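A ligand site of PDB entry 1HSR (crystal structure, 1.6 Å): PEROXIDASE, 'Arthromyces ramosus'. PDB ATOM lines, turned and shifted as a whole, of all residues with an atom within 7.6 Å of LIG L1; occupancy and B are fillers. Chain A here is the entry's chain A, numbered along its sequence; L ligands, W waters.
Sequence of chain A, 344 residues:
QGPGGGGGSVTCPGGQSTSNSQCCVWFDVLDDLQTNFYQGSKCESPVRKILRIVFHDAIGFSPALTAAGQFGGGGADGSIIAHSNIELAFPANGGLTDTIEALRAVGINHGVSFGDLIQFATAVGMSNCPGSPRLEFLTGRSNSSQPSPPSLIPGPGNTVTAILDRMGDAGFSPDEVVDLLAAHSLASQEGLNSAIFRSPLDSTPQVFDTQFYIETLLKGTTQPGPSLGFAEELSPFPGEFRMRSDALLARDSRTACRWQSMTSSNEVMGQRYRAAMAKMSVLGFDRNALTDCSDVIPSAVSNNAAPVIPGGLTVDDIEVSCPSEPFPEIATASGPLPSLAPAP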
ATOM      1  N   ARG A  52      -6.697 -21.972  -6.810  1.00  0.00           N
ATOM      2  CA  ARG A  52      -6.205 -23.195  -6.211  1.00  0.00           C
ATOM      3  C   ARG A  52      -7.241 -24.291  -6.507  1.00  0.00           C
ATOM      4  O   ARG A  52      -6.865 -25.418  -6.857  1.00  0.00           O
ATOM      5  CB  ARG A  52      -6.030 -22.943  -4.714  1.00  0.00           C
ATOM      6  CG  ARG A  52      -5.287 -24.024  -3.956  1.00  0.00           C
ATOM      7  CD  ARG A  52      -4.870 -23.490  -2.596  1.00  0.00           C
ATOM      8  NE  ARG A  52      -4.624 -24.675  -1.830  1.00  0.00           N
ATOM      9  CZ  ARG A  52      -5.091 -24.812  -0.587  1.00  0.00           C
ATOM     10  NH1 ARG A  52      -5.802 -23.863   0.033  1.00  0.00           N
ATOM     11  NH2 ARG A  52      -4.936 -26.005   0.004  1.00  0.00           N
ATOM     12  N   PHE A  55      -7.044 -25.802 -10.250  1.00  0.00           N
ATOM     13  CA  PHE A  55      -5.903 -26.682 -10.363  1.00  0.00           C
ATOM     14  C   PHE A  55      -6.263 -28.023  -9.675  1.00  0.00           C
ATOM     15  O   PHE A  55      -6.114 -29.076 -10.298  1.00  0.00           O
ATOM     16  CB  PHE A  55      -4.664 -26.036  -9.682  1.00  0.00           C
ATOM     17  CG  PHE A  55      -3.408 -26.924  -9.673  1.00  0.00           C
ATOM     18  CD1 PHE A  55      -3.045 -27.648 -10.821  1.00  0.00           C
ATOM     19  CD2 PHE A  55      -2.617 -27.012  -8.527  1.00  0.00           C
ATOM     20  CE1 PHE A  55      -1.903 -28.443 -10.813  1.00  0.00           C
ATOM     21  CE2 PHE A  55      -1.470 -27.811  -8.527  1.00  0.00           C
ATOM     22  CZ  PHE A  55      -1.104 -28.527  -9.665  1.00  0.00           C
ATOM     23  N   HIS A  56      -6.780 -28.029  -8.441  1.00  0.00           N
ATOM     24  CA  HIS A  56      -7.073 -29.279  -7.737  1.00  0.00           C
ATOM     25  C   HIS A  56      -8.219 -30.094  -8.338  1.00  0.00           C
ATOM     26  O   HIS A  56      -8.282 -31.333  -8.194  1.00  0.00           O
ATOM     27  CB  HIS A  56      -7.350 -28.935  -6.272  1.00  0.00           C
ATOM     28  CG  HIS A  56      -6.070 -28.520  -5.545  1.00  0.00           C
ATOM     29  ND1 HIS A  56      -6.000 -28.329  -4.165  1.00  0.00           N
ATOM     30  CD2 HIS A  56      -4.835 -28.221  -6.135  1.00  0.00           C
ATOM     31  CE1 HIS A  56      -4.759 -27.868  -3.932  1.00  0.00           C
ATOM     32  NE2 HIS A  56      -4.069 -27.796  -5.049  1.00  0.00           N
ATOM     33  N   ILE A  59      -6.381 -31.427 -12.088  1.00  0.00           N
ATOM     34  CA  ILE A  59      -5.228 -32.310 -12.014  1.00  0.00           C
ATOM     35  C   ILE A  59      -5.564 -33.716 -11.518  1.00  0.00           C
ATOM     36  O   ILE A  59      -4.685 -34.580 -11.525  1.00  0.00           O
ATOM     37  CB  ILE A  59      -4.132 -31.576 -11.132  1.00  0.00           C
ATOM     38  CG1 ILE A  59      -2.723 -32.071 -11.551  1.00  0.00           C
ATOM     39  CG2 ILE A  59      -4.341 -31.838  -9.633  1.00  0.00           C
ATOM     40  CD1 ILE A  59      -2.369 -31.675 -12.986  1.00  0.00           C
ATOM     41  N   PHE A  90      -8.546 -34.889   1.407  1.00  0.00           N
ATOM     42  CA  PHE A  90      -7.163 -34.986   0.963  1.00  0.00           C
ATOM     43  C   PHE A  90      -6.291 -33.907   1.619  1.00  0.00           C
ATOM     44  O   PHE A  90      -6.737 -32.766   1.729  1.00  0.00           O
ATOM     45  CB  PHE A  90      -7.045 -34.797  -0.537  1.00  0.00           C
ATOM     46  CG  PHE A  90      -7.789 -35.758  -1.450  1.00  0.00           C
ATOM     47  CD1 PHE A  90      -8.356 -36.946  -0.964  1.00  0.00           C
ATOM     48  CD2 PHE A  90      -7.872 -35.421  -2.801  1.00  0.00           C
ATOM     49  CE1 PHE A  90      -9.016 -37.794  -1.875  1.00  0.00           C
ATOM     50  CE2 PHE A  90      -8.528 -36.274  -3.682  1.00  0.00           C
ATOM     51  CZ  PHE A  90      -9.094 -37.462  -3.234  1.00  0.00           C
ATOM     52  N   PRO A  91      -5.022 -34.163   1.959  1.00  0.00           N
ATOM     53  CA  PRO A  91      -4.112 -33.187   2.578  1.00  0.00           C
ATOM     54  C   PRO A  91      -3.992 -31.875   1.816  1.00  0.00           C
ATOM     55  O   PRO A  91      -3.942 -30.780   2.367  1.00  0.00           O
ATOM     56  CB  PRO A  91      -2.782 -33.893   2.660  1.00  0.00           C
ATOM     57  CG  PRO A  91      -3.119 -35.372   2.619  1.00  0.00           C
ATOM     58  CD  PRO A  91      -4.343 -35.439   1.725  1.00  0.00           C
ATOM     59  N   ALA A  92      -3.942 -31.970   0.493  1.00  0.00           N
ATOM     60  CA  ALA A  92      -3.789 -30.799  -0.340  1.00  0.00           C
ATOM     61  C   ALA A  92      -4.999 -29.887  -0.424  1.00  0.00           C
ATOM     62  O   ALA A  92      -4.884 -28.783  -0.963  1.00  0.00           O
ATOM     63  CB  ALA A  92      -3.434 -31.275  -1.740  1.00  0.00           C
ATOM     64  N   ASN A  93      -6.167 -30.327   0.063  1.00  0.00           N
ATOM     65  CA  ASN A  93      -7.383 -29.573  -0.119  1.00  0.00           C
ATOM     66  C   ASN A  93      -7.887 -28.841   1.095  1.00  0.00           C
ATOM     67  O   ASN A  93      -9.082 -28.505   1.201  1.00  0.00           O
ATOM     68  CB  ASN A  93      -8.480 -30.488  -0.650  1.00  0.00           C
ATOM     69  CG  ASN A  93      -8.389 -30.704  -2.164  1.00  0.00           C
ATOM     70  OD1 ASN A  93      -7.978 -29.805  -2.880  1.00  0.00           O
ATOM     71  ND2 ASN A  93      -8.729 -31.856  -2.739  1.00  0.00           N
ATOM     72  N   GLY A  94      -7.000 -28.532   2.020  1.00  0.00           N
ATOM     73  CA  GLY A  94      -7.416 -27.796   3.207  1.00  0.00           C
ATOM     74  C   GLY A  94      -7.648 -26.319   2.891  1.00  0.00           C
ATOM     75  O   GLY A  94      -7.104 -25.754   1.948  1.00  0.00           O
ATOM     76  N   LEU A  96     -10.353 -24.991   1.764  1.00  0.00           N
ATOM     77  CA  LEU A  96     -11.229 -24.777   0.617  1.00  0.00           C
ATOM     78  C   LEU A  96     -12.721 -24.982   0.814  1.00  0.00           C
ATOM     79  O   LEU A  96     -13.531 -24.536  -0.024  1.00  0.00           O
ATOM     80  CB  LEU A  96     -10.780 -25.713  -0.546  1.00  0.00           C
ATOM     81  CG  LEU A  96      -9.355 -25.480  -1.053  1.00  0.00           C
ATOM     82  CD1 LEU A  96      -9.060 -26.469  -2.162  1.00  0.00           C
ATOM     83  CD2 LEU A  96      -9.163 -24.033  -1.488  1.00  0.00           C
ATOM     84  N   ILE A 153      -2.391 -34.648  -6.428  1.00  0.00           N
ATOM     85  CA  ILE A 153      -2.063 -33.246  -6.351  1.00  0.00           C
ATOM     86  C   ILE A 153      -0.634 -33.046  -5.831  1.00  0.00           C
ATOM     87  O   ILE A 153      -0.306 -33.565  -4.749  1.00  0.00           O
ATOM     88  CB  ILE A 153      -3.073 -32.542  -5.429  1.00  0.00           C
ATOM     89  CG1 ILE A 153      -4.492 -32.786  -5.946  1.00  0.00           C
ATOM     90  CG2 ILE A 153      -2.758 -31.030  -5.369  1.00  0.00           C
ATOM     91  CD1 ILE A 153      -5.600 -32.393  -4.966  1.00  0.00           C
ATOM     92  N   PRO A 154       0.241 -32.304  -6.523  1.00  0.00           N
ATOM     93  CA  PRO A 154       1.592 -31.956  -6.063  1.00  0.00           C
ATOM     94  C   PRO A 154       1.575 -31.171  -4.747  1.00  0.00           C
ATOM     95  O   PRO A 154       0.714 -30.298  -4.518  1.00  0.00           O
ATOM     96  CB  PRO A 154       2.189 -31.149  -7.182  1.00  0.00           C
ATOM     97  CG  PRO A 154       1.443 -31.545  -8.412  1.00  0.00           C
ATOM     98  CD  PRO A 154       0.026 -31.847  -7.901  1.00  0.00           C
ATOM     99  N   GLY A 155       2.564 -31.447  -3.895  1.00  0.00           N
ATOM    100  CA  GLY A 155       2.695 -30.779  -2.608  1.00  0.00           C
ATOM    101  C   GLY A 155       3.983 -29.962  -2.526  1.00  0.00           C
ATOM    102  O   GLY A 155       4.949 -30.237  -3.245  1.00  0.00           O
ATOM    103  N   PRO A 156       4.082 -28.953  -1.632  1.00  0.00           N
ATOM    104  CA  PRO A 156       5.228 -28.079  -1.485  1.00  0.00           C
ATOM    105  C   PRO A 156       6.534 -28.718  -0.994  1.00  0.00           C
ATOM    106  O   PRO A 156       7.614 -28.125  -1.117  1.00  0.00           O
ATOM    107  CB  PRO A 156       4.748 -26.993  -0.561  1.00  0.00           C
ATOM    108  CG  PRO A 156       3.792 -27.715   0.353  1.00  0.00           C
ATOM    109  CD  PRO A 156       3.077 -28.636  -0.640  1.00  0.00           C
ATOM    110  N   GLY A 157       6.441 -29.915  -0.418  1.00  0.00           N
ATOM    111  CA  GLY A 157       7.606 -30.651   0.043  1.00  0.00           C
ATOM    112  C   GLY A 157       8.068 -31.678  -0.986  1.00  0.00           C
ATOM    113  O   GLY A 157       9.022 -32.409  -0.740  1.00  0.00           O
ATOM    114  N   ASN A 158       7.435 -31.801  -2.156  1.00  0.00           N
ATOM    115  CA  ASN A 158       7.846 -32.787  -3.161  1.00  0.00           C
ATOM    116  C   ASN A 158       9.107 -32.343  -3.876  1.00  0.00           C
ATOM    117  O   ASN A 158       9.355 -31.146  -3.992  1.00  0.00           O
ATOM    118  CB  ASN A 158       6.806 -32.998  -4.227  1.00  0.00           C
ATOM    119  CG  ASN A 158       5.485 -33.546  -3.746  1.00  0.00           C
ATOM    120  OD1 ASN A 158       4.543 -33.676  -4.518  1.00  0.00           O
ATOM    121  ND2 ASN A 158       5.261 -33.863  -2.481  1.00  0.00           N
ATOM    122  N   HIS A 184       0.958 -18.097  -8.921  1.00  0.00           N
ATOM    123  CA  HIS A 184       1.488 -17.739  -7.606  1.00  0.00           C
ATOM    124  C   HIS A 184       1.828 -16.251  -7.517  1.00  0.00           C
ATOM    125  O   HIS A 184       2.245 -15.724  -6.473  1.00  0.00           O
ATOM    126  CB  HIS A 184       2.706 -18.608  -7.285  1.00  0.00           C
ATOM    127  CG  HIS A 184       2.310 -19.989  -6.748  1.00  0.00           C
ATOM    128  ND1 HIS A 184       3.220 -20.818  -6.105  1.00  0.00           N
ATOM    129  CD2 HIS A 184       1.031 -20.571  -6.747  1.00  0.00           C
ATOM    130  CE1 HIS A 184       2.483 -21.863  -5.706  1.00  0.00           C
ATOM    131  NE2 HIS A 184       1.230 -21.750  -6.024  1.00  0.00           N
ATOM    132  N   GLY A 191      -2.351 -22.072   5.432  1.00  0.00           N
ATOM    133  CA  GLY A 191      -2.203 -23.295   6.200  1.00  0.00           C
ATOM    134  C   GLY A 191      -0.803 -23.834   6.386  1.00  0.00           C
ATOM    135  O   GLY A 191      -0.633 -24.829   7.096  1.00  0.00           O
ATOM    136  N   LEU A 192       0.204 -23.261   5.759  1.00  0.00           N
ATOM    137  CA  LEU A 192       1.569 -23.756   5.915  1.00  0.00           C
ATOM    138  C   LEU A 192       2.206 -23.170   7.157  1.00  0.00           C
ATOM    139  O   LEU A 192       2.996 -23.840   7.824  1.00  0.00           O
ATOM    140  CB  LEU A 192       2.361 -23.383   4.670  1.00  0.00           C
ATOM    141  CG  LEU A 192       2.524 -24.343   3.494  1.00  0.00           C
ATOM    142  CD1 LEU A 192       1.372 -25.255   3.313  1.00  0.00           C
ATOM    143  CD2 LEU A 192       2.785 -23.485   2.293  1.00  0.00           C
ATOM    144  N   PHE A 230       5.435 -25.756   7.454  1.00  0.00           N
ATOM    145  CA  PHE A 230       5.631 -26.896   6.598  1.00  0.00           C
ATOM    146  C   PHE A 230       6.101 -26.399   5.227  1.00  0.00           C
ATOM    147  O   PHE A 230       5.513 -25.501   4.594  1.00  0.00           O
ATOM    148  CB  PHE A 230       4.301 -27.644   6.506  1.00  0.00           C
ATOM    149  CG  PHE A 230       4.386 -28.840   5.577  1.00  0.00           C
ATOM    150  CD1 PHE A 230       5.185 -29.926   5.911  1.00  0.00           C
ATOM    151  CD2 PHE A 230       3.706 -28.806   4.346  1.00  0.00           C
ATOM    152  CE1 PHE A 230       5.333 -30.975   4.990  1.00  0.00           C
ATOM    153  CE2 PHE A 230       3.865 -29.858   3.434  1.00  0.00           C
ATOM    154  CZ  PHE A 230       4.675 -30.936   3.758  1.00  0.00           C
ATOM    155  N   MET A 243       7.775 -20.945  -0.450  1.00  0.00           N
ATOM    156  CA  MET A 243       7.633 -22.383  -0.220  1.00  0.00           C
ATOM    157  C   MET A 243       8.741 -23.127  -0.987  1.00  0.00           C
ATOM    158  O   MET A 243       9.262 -22.650  -2.011  1.00  0.00           O
ATOM    159  CB  MET A 243       6.229 -22.919  -0.660  1.00  0.00           C
ATOM    160  CG  MET A 243       5.826 -22.818  -2.098  1.00  0.00           C
ATOM    161  SD  MET A 243       4.208 -23.583  -2.426  1.00  0.00           S
ATOM    162  CE  MET A 243       4.387 -23.790  -4.123  1.00  0.00           C
HETATM  163  C1  LIG L   1      -1.015 -28.255  -1.442  1.00  0.00           C
HETATM  164  C2  LIG L   1      -1.191 -27.556  -0.223  1.00  0.00           C
HETATM  165  C3  LIG L   1      -0.817 -28.141   0.998  1.00  0.00           C
HETATM  166  C4  LIG L   1      -0.261 -29.425   1.016  1.00  0.00           C
HETATM  167  C5  LIG L   1      -0.096 -30.132  -0.193  1.00  0.00           C
HETATM  168  C6  LIG L   1      -0.468 -29.555  -1.408  1.00  0.00           C
HETATM  169  C7  LIG L   1      -1.397 -27.621  -2.643  1.00  0.00           C
HETATM  170  O1  LIG L   1      -2.132 -26.604  -2.634  1.00  0.00           O
HETATM  171  N1  LIG L   1      -0.950 -28.132  -3.804  1.00  0.00           N
HETATM  172  O2  LIG L   1      -1.380 -27.411  -4.914  1.00  0.00           O
HETATM  173  C1  LG2 L   2      -1.258 -21.455  -2.924  1.00  0.00           C
HETATM  174  C2  LG2 L   2       1.338 -25.437  -3.689  1.00  0.00           C
HETATM  175  C3  LG2 L   2       0.589 -24.955  -8.415  1.00  0.00           C
HETATM  176  C4  LG2 L   2      -2.631 -21.542  -7.542  1.00  0.00           C
HETATM  177  C5  LG2 L   2      -0.480 -22.577  -2.724  1.00  0.00           C
HETATM  178  C6  LG2 L   2      -0.149 -23.104  -1.419  1.00  0.00           C
HETATM  179  C7  LG2 L   2       0.567 -24.256  -1.634  1.00  0.00           C
HETATM  180  C8  LG2 L   2       0.640 -24.426  -3.056  1.00  0.00           C
HETATM  181  C9  LG2 L   2       1.202 -25.177  -0.604  1.00  0.00           C
HETATM  182  C10 LG2 L   2      -0.612 -22.487  -0.118  1.00  0.00           C
HETATM  183  C11 LG2 L   2      -1.946 -23.048   0.349  1.00  0.00           C
HETATM  184  C12 LG2 L   2      -2.284 -22.551   1.735  1.00  0.00           C
HETATM  185  O1  LG2 L   2      -3.139 -21.696   1.863  1.00  0.00           O
HETATM  186  O2  LG2 L   2      -1.657 -22.991   2.707  1.00  0.00           O
HETATM  187  C13 LG2 L   2       1.467 -25.584  -5.065  1.00  0.00           C
HETATM  188  C14 LG2 L   2       2.290 -26.606  -5.708  1.00  0.00           C
HETATM  189  C15 LG2 L   2       2.072 -26.468  -7.058  1.00  0.00           C
HETATM  190  C16 LG2 L   2       1.169 -25.334  -7.210  1.00  0.00           C
HETATM  191  C17 LG2 L   2       3.233 -27.568  -5.000  1.00  0.00           C
HETATM  192  C18 LG2 L   2       2.471 -27.315  -8.093  1.00  0.00           C
HETATM  193  C19 LG2 L   2       3.821 -27.425  -8.562  1.00  0.00           C
HETATM  194  C20 LG2 L   2      -0.411 -24.035  -8.585  1.00  0.00           C
HETATM  195  C21 LG2 L   2      -1.141 -23.847  -9.826  1.00  0.00           C
HETATM  196  C22 LG2 L   2      -2.121 -22.938  -9.571  1.00  0.00           C
HETATM  197  C23 LG2 L   2      -1.941 -22.557  -8.177  1.00  0.00           C
HETATM  198  C24 LG2 L   2      -0.834 -24.599 -11.119  1.00  0.00           C
HETATM  199  C25 LG2 L   2      -3.185 -22.515 -10.379  1.00  0.00           C
HETATM  200  C26 LG2 L   2      -3.144 -22.297 -11.824  1.00  0.00           C
HETATM  201  C27 LG2 L   2      -2.432 -21.130  -6.219  1.00  0.00           C
HETATM  202  C28 LG2 L   2      -3.005 -19.907  -5.653  1.00  0.00           C
HETATM  203  C29 LG2 L   2      -2.632 -19.927  -4.354  1.00  0.00           C
HETATM  204  C30 LG2 L   2      -1.793 -21.081  -4.151  1.00  0.00           C
HETATM  205  C31 LG2 L   2      -3.693 -18.785  -6.426  1.00  0.00           C
HETATM  206  C32 LG2 L   2      -3.001 -18.919  -3.298  1.00  0.00           C
HETATM  207  C33 LG2 L   2      -4.230 -19.294  -2.460  1.00  0.00           C
HETATM  208  C34 LG2 L   2      -4.553 -18.237  -1.405  1.00  0.00           C
HETATM  209  O3  LG2 L   2      -5.450 -18.486  -0.606  1.00  0.00           O
HETATM  210  O4  LG2 L   2      -3.953 -17.156  -1.393  1.00  0.00           O
HETATM  211  N1  LG2 L   2      -0.021 -23.407  -3.720  1.00  0.00           N
HETATM  212  N2  LG2 L   2       0.827 -24.792  -5.991  1.00  0.00           N
HETATM  213  N3  LG2 L   2      -0.927 -23.263  -7.578  1.00  0.00           N
HETATM  214  N4  LG2 L   2      -1.625 -21.779  -5.312  1.00  0.00           N
HETATM  215 FE1  LG2 L   2      -0.342 -23.238  -5.669  1.00  0.00          FE
HETATM  216  O   HOH W   1      -2.348 -25.019  -5.206  1.00  0.00           O
HETATM  217  O   HOH W   2      -4.114 -28.043   2.138  1.00  0.00           O
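NE2 of His 56 sits at hydrogen-bond distance from O2 of LIG L1 (2.7 Å).
The backbone carbonyl oxygen (O) of Pro 154 sits at hydrogen-bond distance from a nitrogen (N1) of LIG L1 (2.8 Å).
NE of Arg 52 lies within hydrogen-bond range of O1 of LIG L1 (3.3 Å).
O1 of LG2 L2 is in salt-bridge range of NH1 of Arg 52 (3.9 Å).
A ring nitrogen (NE2) of His 184 binds an iron atom (FE1) of LG2 L2 (2.2 Å).
The backbone NH (N) of Gly 191 lies within hydrogen-bond range of an oxygen (O2) of LG2 L2 (3.0 Å).
The backbone carbonyl oxygen (O) of Ala 92 sits close to a ring nitrogen (ND1) of His 56 (3.4 Å).
OD1 of Asn 93 lies within hydrogen-bond range of ND1 of His 56 (2.8 Å).
The backbone carbonyl oxygen (O) of Ala 92 sits at hydrogen-bond distance from the guanidinium group (NH2) of Arg 52, at 2.9 Å.
The guanidinium group (NH2) of Arg 52 lies within hydrogen-bond range of the backbone carbonyl oxygen (O) of Gly 94 (2.9 Å).
N of Gly 155 sits at hydrogen-bond distance from OD1 of Asn 158 (3.0 Å).
Merely in contact with LIG L1: Phe 55 (3.6 Å), Ala 92 (3.4 Å), Ile 153 (3.8 Å), Gly 155 (3.6 Å) and Pro 156 (3.5 Å).
Hydrophobic or aromatic side chains within 4 Å of LIG L1: Phe 55, His 56, Ala 92, Ile 153 and Pro 156.
Water W1 bridges an oxygen (O2) of LIG L1 (2.6 Å) and a ring nitrogen (NE2) of His 56 (3.3 Å).
Water W2 lies within hydrogen-bond range of O of Pro 91 (2.8 Å), N of Gly 94 (2.9 Å), NH2 of Arg 52 (3.1 Å) and O of Ala 92 (3.3 Å).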
